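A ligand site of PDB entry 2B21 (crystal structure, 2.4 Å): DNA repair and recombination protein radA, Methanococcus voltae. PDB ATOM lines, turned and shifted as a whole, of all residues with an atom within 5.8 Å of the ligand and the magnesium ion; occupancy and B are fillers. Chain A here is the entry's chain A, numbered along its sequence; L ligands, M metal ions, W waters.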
ATOM      1  N   GLY A 105      16.314   1.039  10.377  1.00  0.00           N
ATOM      2  CA  GLY A 105      17.565   1.751  10.414  1.00  0.00           C
ATOM      3  C   GLY A 105      17.431   3.188   9.992  1.00  0.00           C
ATOM      4  O   GLY A 105      16.461   3.573   9.318  1.00  0.00           O
ATOM      5  N   VAL A 106      18.415   3.985  10.395  1.00  0.00           N
ATOM      6  CA  VAL A 106      18.449   5.402  10.068  1.00  0.00           C
ATOM      7  C   VAL A 106      18.744   5.565   8.590  1.00  0.00           C
ATOM      8  O   VAL A 106      19.223   4.629   7.941  1.00  0.00           O
ATOM      9  CB  VAL A 106      19.542   6.120  10.883  1.00  0.00           C
ATOM     10  CG1 VAL A 106      19.303   5.918  12.376  1.00  0.00           C
ATOM     11  CG2 VAL A 106      20.914   5.598  10.499  1.00  0.00           C
ATOM     12  N   PHE A 107      18.442   6.737   8.044  1.00  0.00           N
ATOM     13  CA  PHE A 107      18.705   7.035   6.641  1.00  0.00           C
ATOM     14  C   PHE A 107      20.131   6.601   6.265  1.00  0.00           C
ATOM     15  O   PHE A 107      21.088   6.934   6.953  1.00  0.00           O
ATOM     16  CB  PHE A 107      18.575   8.537   6.376  1.00  0.00           C
ATOM     17  CG  PHE A 107      17.158   9.040   6.407  1.00  0.00           C
ATOM     18  CD1 PHE A 107      16.263   8.697   5.405  1.00  0.00           C
ATOM     19  CD2 PHE A 107      16.715   9.846   7.455  1.00  0.00           C
ATOM     20  CE1 PHE A 107      14.943   9.150   5.439  1.00  0.00           C
ATOM     21  CE2 PHE A 107      15.404  10.303   7.499  1.00  0.00           C
ATOM     22  CZ  PHE A 107      14.514   9.952   6.486  1.00  0.00           C
ATOM     23  N   GLY A 108      20.243   5.855   5.170  1.00  0.00           N
ATOM     24  CA  GLY A 108      21.542   5.408   4.685  1.00  0.00           C
ATOM     25  C   GLY A 108      22.274   4.334   5.474  1.00  0.00           C
ATOM     26  O   GLY A 108      23.455   4.083   5.212  1.00  0.00           O
ATOM     27  N   SER A 109      21.608   3.700   6.428  1.00  0.00           N
ATOM     28  CA  SER A 109      22.274   2.680   7.224  1.00  0.00           C
ATOM     29  C   SER A 109      22.563   1.370   6.490  1.00  0.00           C
ATOM     30  O   SER A 109      23.292   0.545   7.003  1.00  0.00           O
ATOM     31  CB  SER A 109      21.485   2.389   8.508  1.00  0.00           C
ATOM     32  OG  SER A 109      20.134   2.075   8.232  1.00  0.00           O
ATOM     33  N   GLY A 110      21.976   1.186   5.317  1.00  0.00           N
ATOM     34  CA  GLY A 110      22.232  -0.022   4.534  1.00  0.00           C
ATOM     35  C   GLY A 110      21.066  -0.976   4.319  1.00  0.00           C
ATOM     36  O   GLY A 110      21.240  -2.071   3.760  1.00  0.00           O
ATOM     37  N   LYS A 111      19.871  -0.569   4.758  1.00  0.00           N
ATOM     38  CA  LYS A 111      18.681  -1.385   4.628  1.00  0.00           C
ATOM     39  C   LYS A 111      18.579  -2.034   3.246  1.00  0.00           C
ATOM     40  O   LYS A 111      18.497  -3.254   3.122  1.00  0.00           O
ATOM     41  CB  LYS A 111      17.444  -0.520   4.884  1.00  0.00           C
ATOM     42  CG  LYS A 111      17.432   0.171   6.242  1.00  0.00           C
ATOM     43  CD  LYS A 111      16.108   0.862   6.492  1.00  0.00           C
ATOM     44  CE  LYS A 111      15.984   2.142   5.681  1.00  0.00           C
ATOM     45  NZ  LYS A 111      16.920   3.162   6.209  1.00  0.00           N
ATOM     46  N   THR A 112      18.585  -1.198   2.216  1.00  0.00           N
ATOM     47  CA  THR A 112      18.481  -1.640   0.836  1.00  0.00           C
ATOM     48  C   THR A 112      19.638  -2.555   0.415  1.00  0.00           C
ATOM     49  O   THR A 112      19.424  -3.539  -0.305  1.00  0.00           O
ATOM     50  CB  THR A 112      18.385  -0.402  -0.071  1.00  0.00           C
ATOM     51  OG1 THR A 112      17.239   0.351   0.312  1.00  0.00           O
ATOM     52  CG2 THR A 112      18.277  -0.788  -1.556  1.00  0.00           C
ATOM     53  N   GLN A 113      20.849  -2.248   0.864  1.00  0.00           N
ATOM     54  CA  GLN A 113      22.012  -3.078   0.543  1.00  0.00           C
ATOM     55  C   GLN A 113      21.789  -4.516   1.023  1.00  0.00           C
ATOM     56  O   GLN A 113      22.066  -5.476   0.295  1.00  0.00           O
ATOM     57  CB  GLN A 113      23.286  -2.530   1.207  1.00  0.00           C
ATOM     58  CG  GLN A 113      23.677  -1.146   0.718  1.00  0.00           C
ATOM     59  CD  GLN A 113      23.693  -1.056  -0.792  1.00  0.00           C
ATOM     60  OE1 GLN A 113      24.553  -1.649  -1.454  1.00  0.00           O
ATOM     61  NE2 GLN A 113      22.740  -0.317  -1.359  1.00  0.00           N
ATOM     62  N   ILE A 114      21.305  -4.653   2.256  1.00  0.00           N
ATOM     63  CA  ILE A 114      21.059  -5.954   2.841  1.00  0.00           C
ATOM     64  C   ILE A 114      20.040  -6.721   2.009  1.00  0.00           C
ATOM     65  O   ILE A 114      20.154  -7.938   1.821  1.00  0.00           O
ATOM     66  CB  ILE A 114      20.600  -5.804   4.304  1.00  0.00           C
ATOM     67  CG1 ILE A 114      21.724  -5.162   5.131  1.00  0.00           C
ATOM     68  CG2 ILE A 114      20.209  -7.153   4.897  1.00  0.00           C
ATOM     69  CD1 ILE A 114      21.374  -4.856   6.578  1.00  0.00           C
ATOM     70  N   GLU A 151      10.528   2.084  -2.788  1.00  0.00           N
ATOM     71  CA  GLU A 151      11.328   3.304  -2.860  1.00  0.00           C
ATOM     72  C   GLU A 151      11.820   3.705  -4.247  1.00  0.00           C
ATOM     73  O   GLU A 151      12.054   4.882  -4.513  1.00  0.00           O
ATOM     74  CB  GLU A 151      12.549   3.171  -1.944  1.00  0.00           C
ATOM     75  CG  GLU A 151      12.253   2.626  -0.556  1.00  0.00           C
ATOM     76  CD  GLU A 151      11.317   3.529   0.250  1.00  0.00           C
ATOM     77  OE1 GLU A 151      11.604   3.737   1.452  1.00  0.00           O
ATOM     78  OE2 GLU A 151      10.297   3.997  -0.294  1.00  0.00           O
ATOM     79  N   THR A 153      14.534   2.184  -5.415  1.00  0.00           N
ATOM     80  CA  THR A 153      15.972   2.043  -5.279  1.00  0.00           C
ATOM     81  C   THR A 153      16.529   0.678  -5.622  1.00  0.00           C
ATOM     82  O   THR A 153      17.603   0.304  -5.140  1.00  0.00           O
ATOM     83  CB  THR A 153      16.450   2.428  -3.872  1.00  0.00           C
ATOM     84  OG1 THR A 153      15.628   1.784  -2.895  1.00  0.00           O
ATOM     85  CG2 THR A 153      16.393   3.954  -3.683  1.00  0.00           C
ATOM     86  N   ARG A 158      24.038  -2.884  -8.901  1.00  0.00           N
ATOM     87  CA  ARG A 158      24.481  -3.272  -7.572  1.00  0.00           C
ATOM     88  C   ARG A 158      24.383  -4.791  -7.375  1.00  0.00           C
ATOM     89  O   ARG A 158      25.162  -5.393  -6.648  1.00  0.00           O
ATOM     90  CB  ARG A 158      23.646  -2.524  -6.522  1.00  0.00           C
ATOM     91  CG  ARG A 158      24.218  -2.592  -5.134  1.00  0.00           C
ATOM     92  CD  ARG A 158      25.610  -1.990  -5.061  1.00  0.00           C
ATOM     93  NE  ARG A 158      26.124  -2.098  -3.705  1.00  0.00           N
ATOM     94  CZ  ARG A 158      27.349  -2.506  -3.390  1.00  0.00           C
ATOM     95  NH1 ARG A 158      27.712  -2.563  -2.117  1.00  0.00           N
ATOM     96  NH2 ARG A 158      28.206  -2.849  -4.338  1.00  0.00           N
ATOM     97  N   GLN A 161      27.446  -6.251  -9.278  1.00  0.00           N
ATOM     98  CA  GLN A 161      28.673  -6.013  -8.545  1.00  0.00           C
ATOM     99  C   GLN A 161      28.798  -6.914  -7.313  1.00  0.00           C
ATOM    100  O   GLN A 161      29.838  -7.499  -7.063  1.00  0.00           O
ATOM    101  CB  GLN A 161      28.715  -4.535  -8.153  1.00  0.00           C
ATOM    102  CG  GLN A 161      29.908  -4.119  -7.330  1.00  0.00           C
ATOM    103  CD  GLN A 161      29.968  -2.618  -7.157  1.00  0.00           C
ATOM    104  OE1 GLN A 161      28.944  -1.928  -7.235  1.00  0.00           O
ATOM    105  NE2 GLN A 161      31.169  -2.096  -6.917  1.00  0.00           N
ATOM    106  N   ASP A 211      10.964  -3.563   0.422  1.00  0.00           N
ATOM    107  CA  ASP A 211      11.785  -2.383   0.697  1.00  0.00           C
ATOM    108  C   ASP A 211      11.099  -1.214   0.008  1.00  0.00           C
ATOM    109  O   ASP A 211      11.159  -1.097  -1.218  1.00  0.00           O
ATOM    110  CB  ASP A 211      13.196  -2.595   0.123  1.00  0.00           C
ATOM    111  CG  ASP A 211      14.135  -1.443   0.413  1.00  0.00           C
ATOM    112  OD1 ASP A 211      14.127  -0.909   1.555  1.00  0.00           O
ATOM    113  OD2 ASP A 211      14.917  -1.061  -0.489  1.00  0.00           O
ATOM    114  N   GLN A 257      12.215   2.487   7.907  1.00  0.00           N
ATOM    115  CA  GLN A 257      12.976   3.691   8.186  1.00  0.00           C
ATOM    116  C   GLN A 257      12.618   4.241   9.567  1.00  0.00           C
ATOM    117  O   GLN A 257      11.479   4.621   9.821  1.00  0.00           O
ATOM    118  CB  GLN A 257      12.684   4.735   7.103  1.00  0.00           C
ATOM    119  CG  GLN A 257      13.034   6.154   7.503  1.00  0.00           C
ATOM    120  CD  GLN A 257      14.507   6.334   7.732  1.00  0.00           C
ATOM    121  OE1 GLN A 257      14.928   7.081   8.615  1.00  0.00           O
ATOM    122  NE2 GLN A 257      15.311   5.646   6.921  1.00  0.00           N
ATOM    123  N   LYS A 290      24.977   3.554  11.159  1.00  0.00           N
ATOM    124  CA  LYS A 290      26.299   3.709  10.564  1.00  0.00           C
ATOM    125  C   LYS A 290      27.384   3.830  11.620  1.00  0.00           C
ATOM    126  O   LYS A 290      27.204   4.476  12.646  1.00  0.00           O
ATOM    127  CB  LYS A 290      26.368   4.956   9.686  1.00  0.00           C
ATOM    128  CG  LYS A 290      25.433   5.006   8.484  1.00  0.00           C
ATOM    129  CD  LYS A 290      25.739   6.276   7.663  1.00  0.00           C
ATOM    130  CE  LYS A 290      24.669   6.578   6.610  1.00  0.00           C
ATOM    131  NZ  LYS A 290      24.877   7.893   5.917  1.00  0.00           N
ATOM    132  N   ARG A 296      29.061  -0.692  10.104  1.00  0.00           N
ATOM    133  CA  ARG A 296      27.623  -0.716  10.302  1.00  0.00           C
ATOM    134  C   ARG A 296      27.351  -1.523  11.572  1.00  0.00           C
ATOM    135  O   ARG A 296      28.030  -2.509  11.839  1.00  0.00           O
ATOM    136  CB  ARG A 296      26.926  -1.400   9.120  1.00  0.00           C
ATOM    137  CG  ARG A 296      27.135  -0.704   7.800  1.00  0.00           C
ATOM    138  CD  ARG A 296      26.346   0.589   7.738  1.00  0.00           C
ATOM    139  NE  ARG A 296      26.492   1.235   6.434  1.00  0.00           N
ATOM    140  CZ  ARG A 296      27.372   2.199   6.173  1.00  0.00           C
ATOM    141  NH1 ARG A 296      28.191   2.620   7.125  1.00  0.00           N
ATOM    142  NH2 ARG A 296      27.440   2.712   4.948  1.00  0.00           N
ATOM    143  N   ILE A 315      29.866  -2.351   4.688  1.00  0.00           N
ATOM    144  CA  ILE A 315      29.335  -2.379   3.338  1.00  0.00           C
ATOM    145  C   ILE A 315      30.407  -1.778   2.453  1.00  0.00           C
ATOM    146  O   ILE A 315      30.821  -0.645   2.651  1.00  0.00           O
ATOM    147  CB  ILE A 315      28.036  -1.564   3.228  1.00  0.00           C
ATOM    148  CG1 ILE A 315      26.973  -2.143   4.166  1.00  0.00           C
ATOM    149  CG2 ILE A 315      27.531  -1.591   1.788  1.00  0.00           C
ATOM    150  CD1 ILE A 315      25.677  -1.364   4.183  1.00  0.00           C
ATOM    151  N   THR A 316      30.855  -2.556   1.479  1.00  0.00           N
ATOM    152  CA  THR A 316      31.898  -2.107   0.568  1.00  0.00           C
ATOM    153  C   THR A 316      31.395  -2.366  -0.846  1.00  0.00           C
ATOM    154  O   THR A 316      30.224  -2.657  -1.033  1.00  0.00           O
ATOM    155  CB  THR A 316      33.188  -2.873   0.814  1.00  0.00           C
ATOM    156  OG1 THR A 316      32.976  -4.258   0.485  1.00  0.00           O
ATOM    157  CG2 THR A 316      33.586  -2.759   2.275  1.00  0.00           C
ATOM    158  N   GLU A 317      32.284  -2.271  -1.830  1.00  0.00           N
ATOM    159  CA  GLU A 317      31.893  -2.506  -3.214  1.00  0.00           C
ATOM    160  C   GLU A 317      31.444  -3.947  -3.403  1.00  0.00           C
ATOM    161  O   GLU A 317      30.809  -4.283  -4.400  1.00  0.00           O
ATOM    162  CB  GLU A 317      33.049  -2.195  -4.171  1.00  0.00           C
ATOM    163  CG  GLU A 317      34.380  -1.809  -3.515  1.00  0.00           C
ATOM    164  CD  GLU A 317      35.153  -2.986  -2.929  1.00  0.00           C
ATOM    165  OE1 GLU A 317      35.486  -3.922  -3.696  1.00  0.00           O
ATOM    166  OE2 GLU A 317      35.432  -2.969  -1.716  1.00  0.00           O
ATOM    167  N   LYS A 318      31.783  -4.802  -2.432  1.00  0.00           N
ATOM    168  CA  LYS A 318      31.429  -6.216  -2.500  1.00  0.00           C
ATOM    169  C   LYS A 318      30.103  -6.533  -1.821  1.00  0.00           C
ATOM    170  O   LYS A 318      29.610  -7.655  -1.896  1.00  0.00           O
ATOM    171  CB  LYS A 318      32.545  -7.045  -1.865  1.00  0.00           C
ATOM    172  CG  LYS A 318      33.914  -6.731  -2.404  1.00  0.00           C
ATOM    173  CD  LYS A 318      35.001  -7.474  -1.658  1.00  0.00           C
ATOM    174  CE  LYS A 318      36.374  -7.029  -2.114  1.00  0.00           C
ATOM    175  NZ  LYS A 318      37.431  -7.701  -1.330  1.00  0.00           N
HETATM  176  P1  LIG L   1      17.536   4.948   2.811  1.00  0.00           P
HETATM  177  O1  LIG L   1      17.058   5.184   4.142  1.00  0.00           O
HETATM  178  O2  LIG L   1      16.637   3.957   2.114  1.00  0.00           O
HETATM  179  O3  LIG L   1      17.514   6.186   2.064  1.00  0.00           O
HETATM  180  P2  LIG L   1      19.447   2.877   3.201  1.00  0.00           P
HETATM  181  O4  LIG L   1      18.610   1.946   2.379  1.00  0.00           O
HETATM  182  O5  LIG L   1      19.246   2.590   4.614  1.00  0.00           O
HETATM  183  N1  LIG L   1      19.092   4.374   2.880  1.00  0.00           N
HETATM  184  P3  LIG L   1      21.461   2.035   1.423  1.00  0.00           P
HETATM  185  O6  LIG L   1      21.067   0.548   1.389  1.00  0.00           O
HETATM  186  O7  LIG L   1      20.813   2.755   0.304  1.00  0.00           O
HETATM  187  O8  LIG L   1      21.010   2.667   2.845  1.00  0.00           O
HETATM  188  O9  LIG L   1      23.089   2.124   1.298  1.00  0.00           O
HETATM  189  C1  LIG L   1      23.801   3.432   1.026  1.00  0.00           C
HETATM  190  C2  LIG L   1      25.099   3.210   1.187  1.00  0.00           C
HETATM  191  O10 LIG L   1      25.489   1.963   0.497  1.00  0.00           O
HETATM  192  C3  LIG L   1      25.945   4.269   0.434  1.00  0.00           C
HETATM  193  O11 LIG L   1      25.836   5.562   0.891  1.00  0.00           O
HETATM  194  C4  LIG L   1      27.284   3.532   0.159  1.00  0.00           C
HETATM  195  O12 LIG L   1      28.223   3.762   1.350  1.00  0.00           O
HETATM  196  C5  LIG L   1      26.899   2.047   0.155  1.00  0.00           C
HETATM  197  N2  LIG L   1      27.060   1.637  -1.117  1.00  0.00           N
HETATM  198  C6  LIG L   1      26.069   1.528  -2.114  1.00  0.00           C
HETATM  199  N3  LIG L   1      26.608   1.127  -3.212  1.00  0.00           N
HETATM  200  C7  LIG L   1      27.939   0.967  -3.025  1.00  0.00           C
HETATM  201  C8  LIG L   1      28.975   0.583  -3.840  1.00  0.00           C
HETATM  202  N4  LIG L   1      28.741   0.265  -5.135  1.00  0.00           N
HETATM  203  N5  LIG L   1      30.276   0.517  -3.311  1.00  0.00           N
HETATM  204  C9  LIG L   1      30.533   0.850  -1.945  1.00  0.00           C
HETATM  205  N6  LIG L   1      29.537   1.244  -1.119  1.00  0.00           N
HETATM  206  C10 LIG L   1      28.232   1.281  -1.712  1.00  0.00           C
HETATM  207 MG    MG M   1      16.963   2.303   1.243  1.00  0.00          MG
HETATM  208  O   HOH W   1      15.540   2.694  -0.306  1.00  0.00           O
HETATM  209  O   HOH W   2      24.982   5.901   3.699  1.00  0.00           O
HETATM  210  O   HOH W   3      18.187   2.947  -0.375  1.00  0.00           O
HETATM  211  O   HOH W   4      14.397   5.411   4.181  1.00  0.00           O
HETATM  212  O   HOH W   5      24.532   2.054   3.955  1.00  0.00           O
HETATM  213  O   HOH W   6      17.648   5.772  -0.606  1.00  0.00           O
HETATM  214  O   HOH W   7      19.193   7.864   3.217  1.00  0.00           O
HETATM  215  O   HOH W   8      13.564   2.997   3.346  1.00  0.00           O
HETATM  216  O   HOH W   9      14.241   4.925   0.514  1.00  0.00           O
HETATM  217  O   HOH W  10      15.337   1.286   2.329  1.00  0.00           O
HETATM  218  O   HOH W  11      15.812   8.497   2.015  1.00  0.00           O
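An oxygen (O6) of the ligand lies within hydrogen-bond range of the backbone NH of Thr 112 (3.1 Å). An oxygen (O6) of the ligand sits at hydrogen-bond distance from the backbone NH of Gln 113, at 2.9 Å. NE2 of Gln 113 sits close to O6 of the ligand (3.3 Å). The backbone NH (N) of Lys 111 lies within hydrogen-bond range of an oxygen (O5) of the ligand (3.2 Å). An oxygen (O5) of the ligand lies within salt-bridge range of the side-chain amino group (NZ) of Lys 111 (2.9 Å). An oxygen (O1) of the ligand is in hydrogen-bond range of the backbone NH (N) of Gly 108 (3.4 Å). The backbone NH of Gly 110 sits at hydrogen-bond distance from an oxygen (O8) of the ligand (3.0 Å). The side-chain amide oxygen (OE1) of Gln 161 lies within hydrogen-bond range of a nitrogen (N4) of the ligand, 3.0 Å away. N of Ser 109 is in hydrogen-bond range of O5 of the ligand, at 3.2 Å. A nitrogen (N3) of the ligand lies within hydrogen-bond range of the guanidinium group (NE) of Arg 158, at 3.3 Å. O1 of the ligand lies within hydrogen-bond range of NE2 of Gln 257.
Within 4 Å of the magnesium ion: Thr 112. The nearest printed residue that does not touch the magnesium ion is Asp 211 (4.3 Å).
Residues that only touch the ligand: Glu 317 (3.4 Å), Thr 316 (3.5 Å), Phe 107 (3.5 Å), Arg 296 (3.8 Å) and Val 106 (3.9 Å). Hydrophobic or aromatic side chains that line the ligand: Phe 107. Within 4 Å of the ligand: Val 106, Phe 107, Gly 108, Ser 109, Gly 110, Lys 111, Thr 112, Gln 113, Arg 158, Gln 161, Gln 257, Arg 296, Thr 316 and Glu 317. The nearest printed residue that does not touch the ligand is Ile 315 (4.04 Å).
Water W7 lies within hydrogen-bond range of an oxygen (O3) of the ligand (2.6 Å) and the backbone NH (N) of Gly 108 (3.0 Å). Water W4 bridges an oxygen (O1) of the ligand and the side-chain amide nitrogen of Gln 257. Water W2 lies within hydrogen-bond range of O of Gly 108 (2.8 Å), O11 of the ligand (3.0 Å) and NZ of Lys 290 (3.0 Å). Water W5 lies within hydrogen-bond range of O of Gly 108 (2.6 Å), N of Gly 110 (3.0 Å), O9 of the ligand (3.0 Å) and NH2 of Arg 296 (3.1 Å).
OD2 of Asp 211 lies close to OG1 of Thr 112 (2.8 Å). The guanidinium group (NE) of Arg 158 is in hydrogen-bond range of the side-chain amide oxygen (OE1) of Gln 113 (2.8 Å). NZ of Lys 111 sits close to NE2 of Gln 257 (3.0 Å). O of Val 106 sits at hydrogen-bond distance from NZ of Lys 111. The guanidinium group (NH2) of Arg 158 sits at hydrogen-bond distance from the side-chain amide oxygen (OE1) of Gln 161 (3.1 Å). The guanidinium group (NH2) of Arg 158 is in hydrogen-bond range of the backbone carbonyl oxygen (O) of Glu 317, at 3.0 Å. NH1 of Arg 158 lies within hydrogen-bond range of O of Thr 316, at 2.7 Å. NE2 of Gln 257 lies within hydrogen-bond range of O of Gly 105, 3.4 Å away.
The magnesium ion is bound by an oxygen (O2) of the ligand (1.9 Å), an oxygen (O4) of the ligand (2.0 Å), water W3 (2.1 Å), water W1 (2.1 Å), the side-chain hydroxyl of Thr 112 (2.2 Å) and water W10 (2.2 Å).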
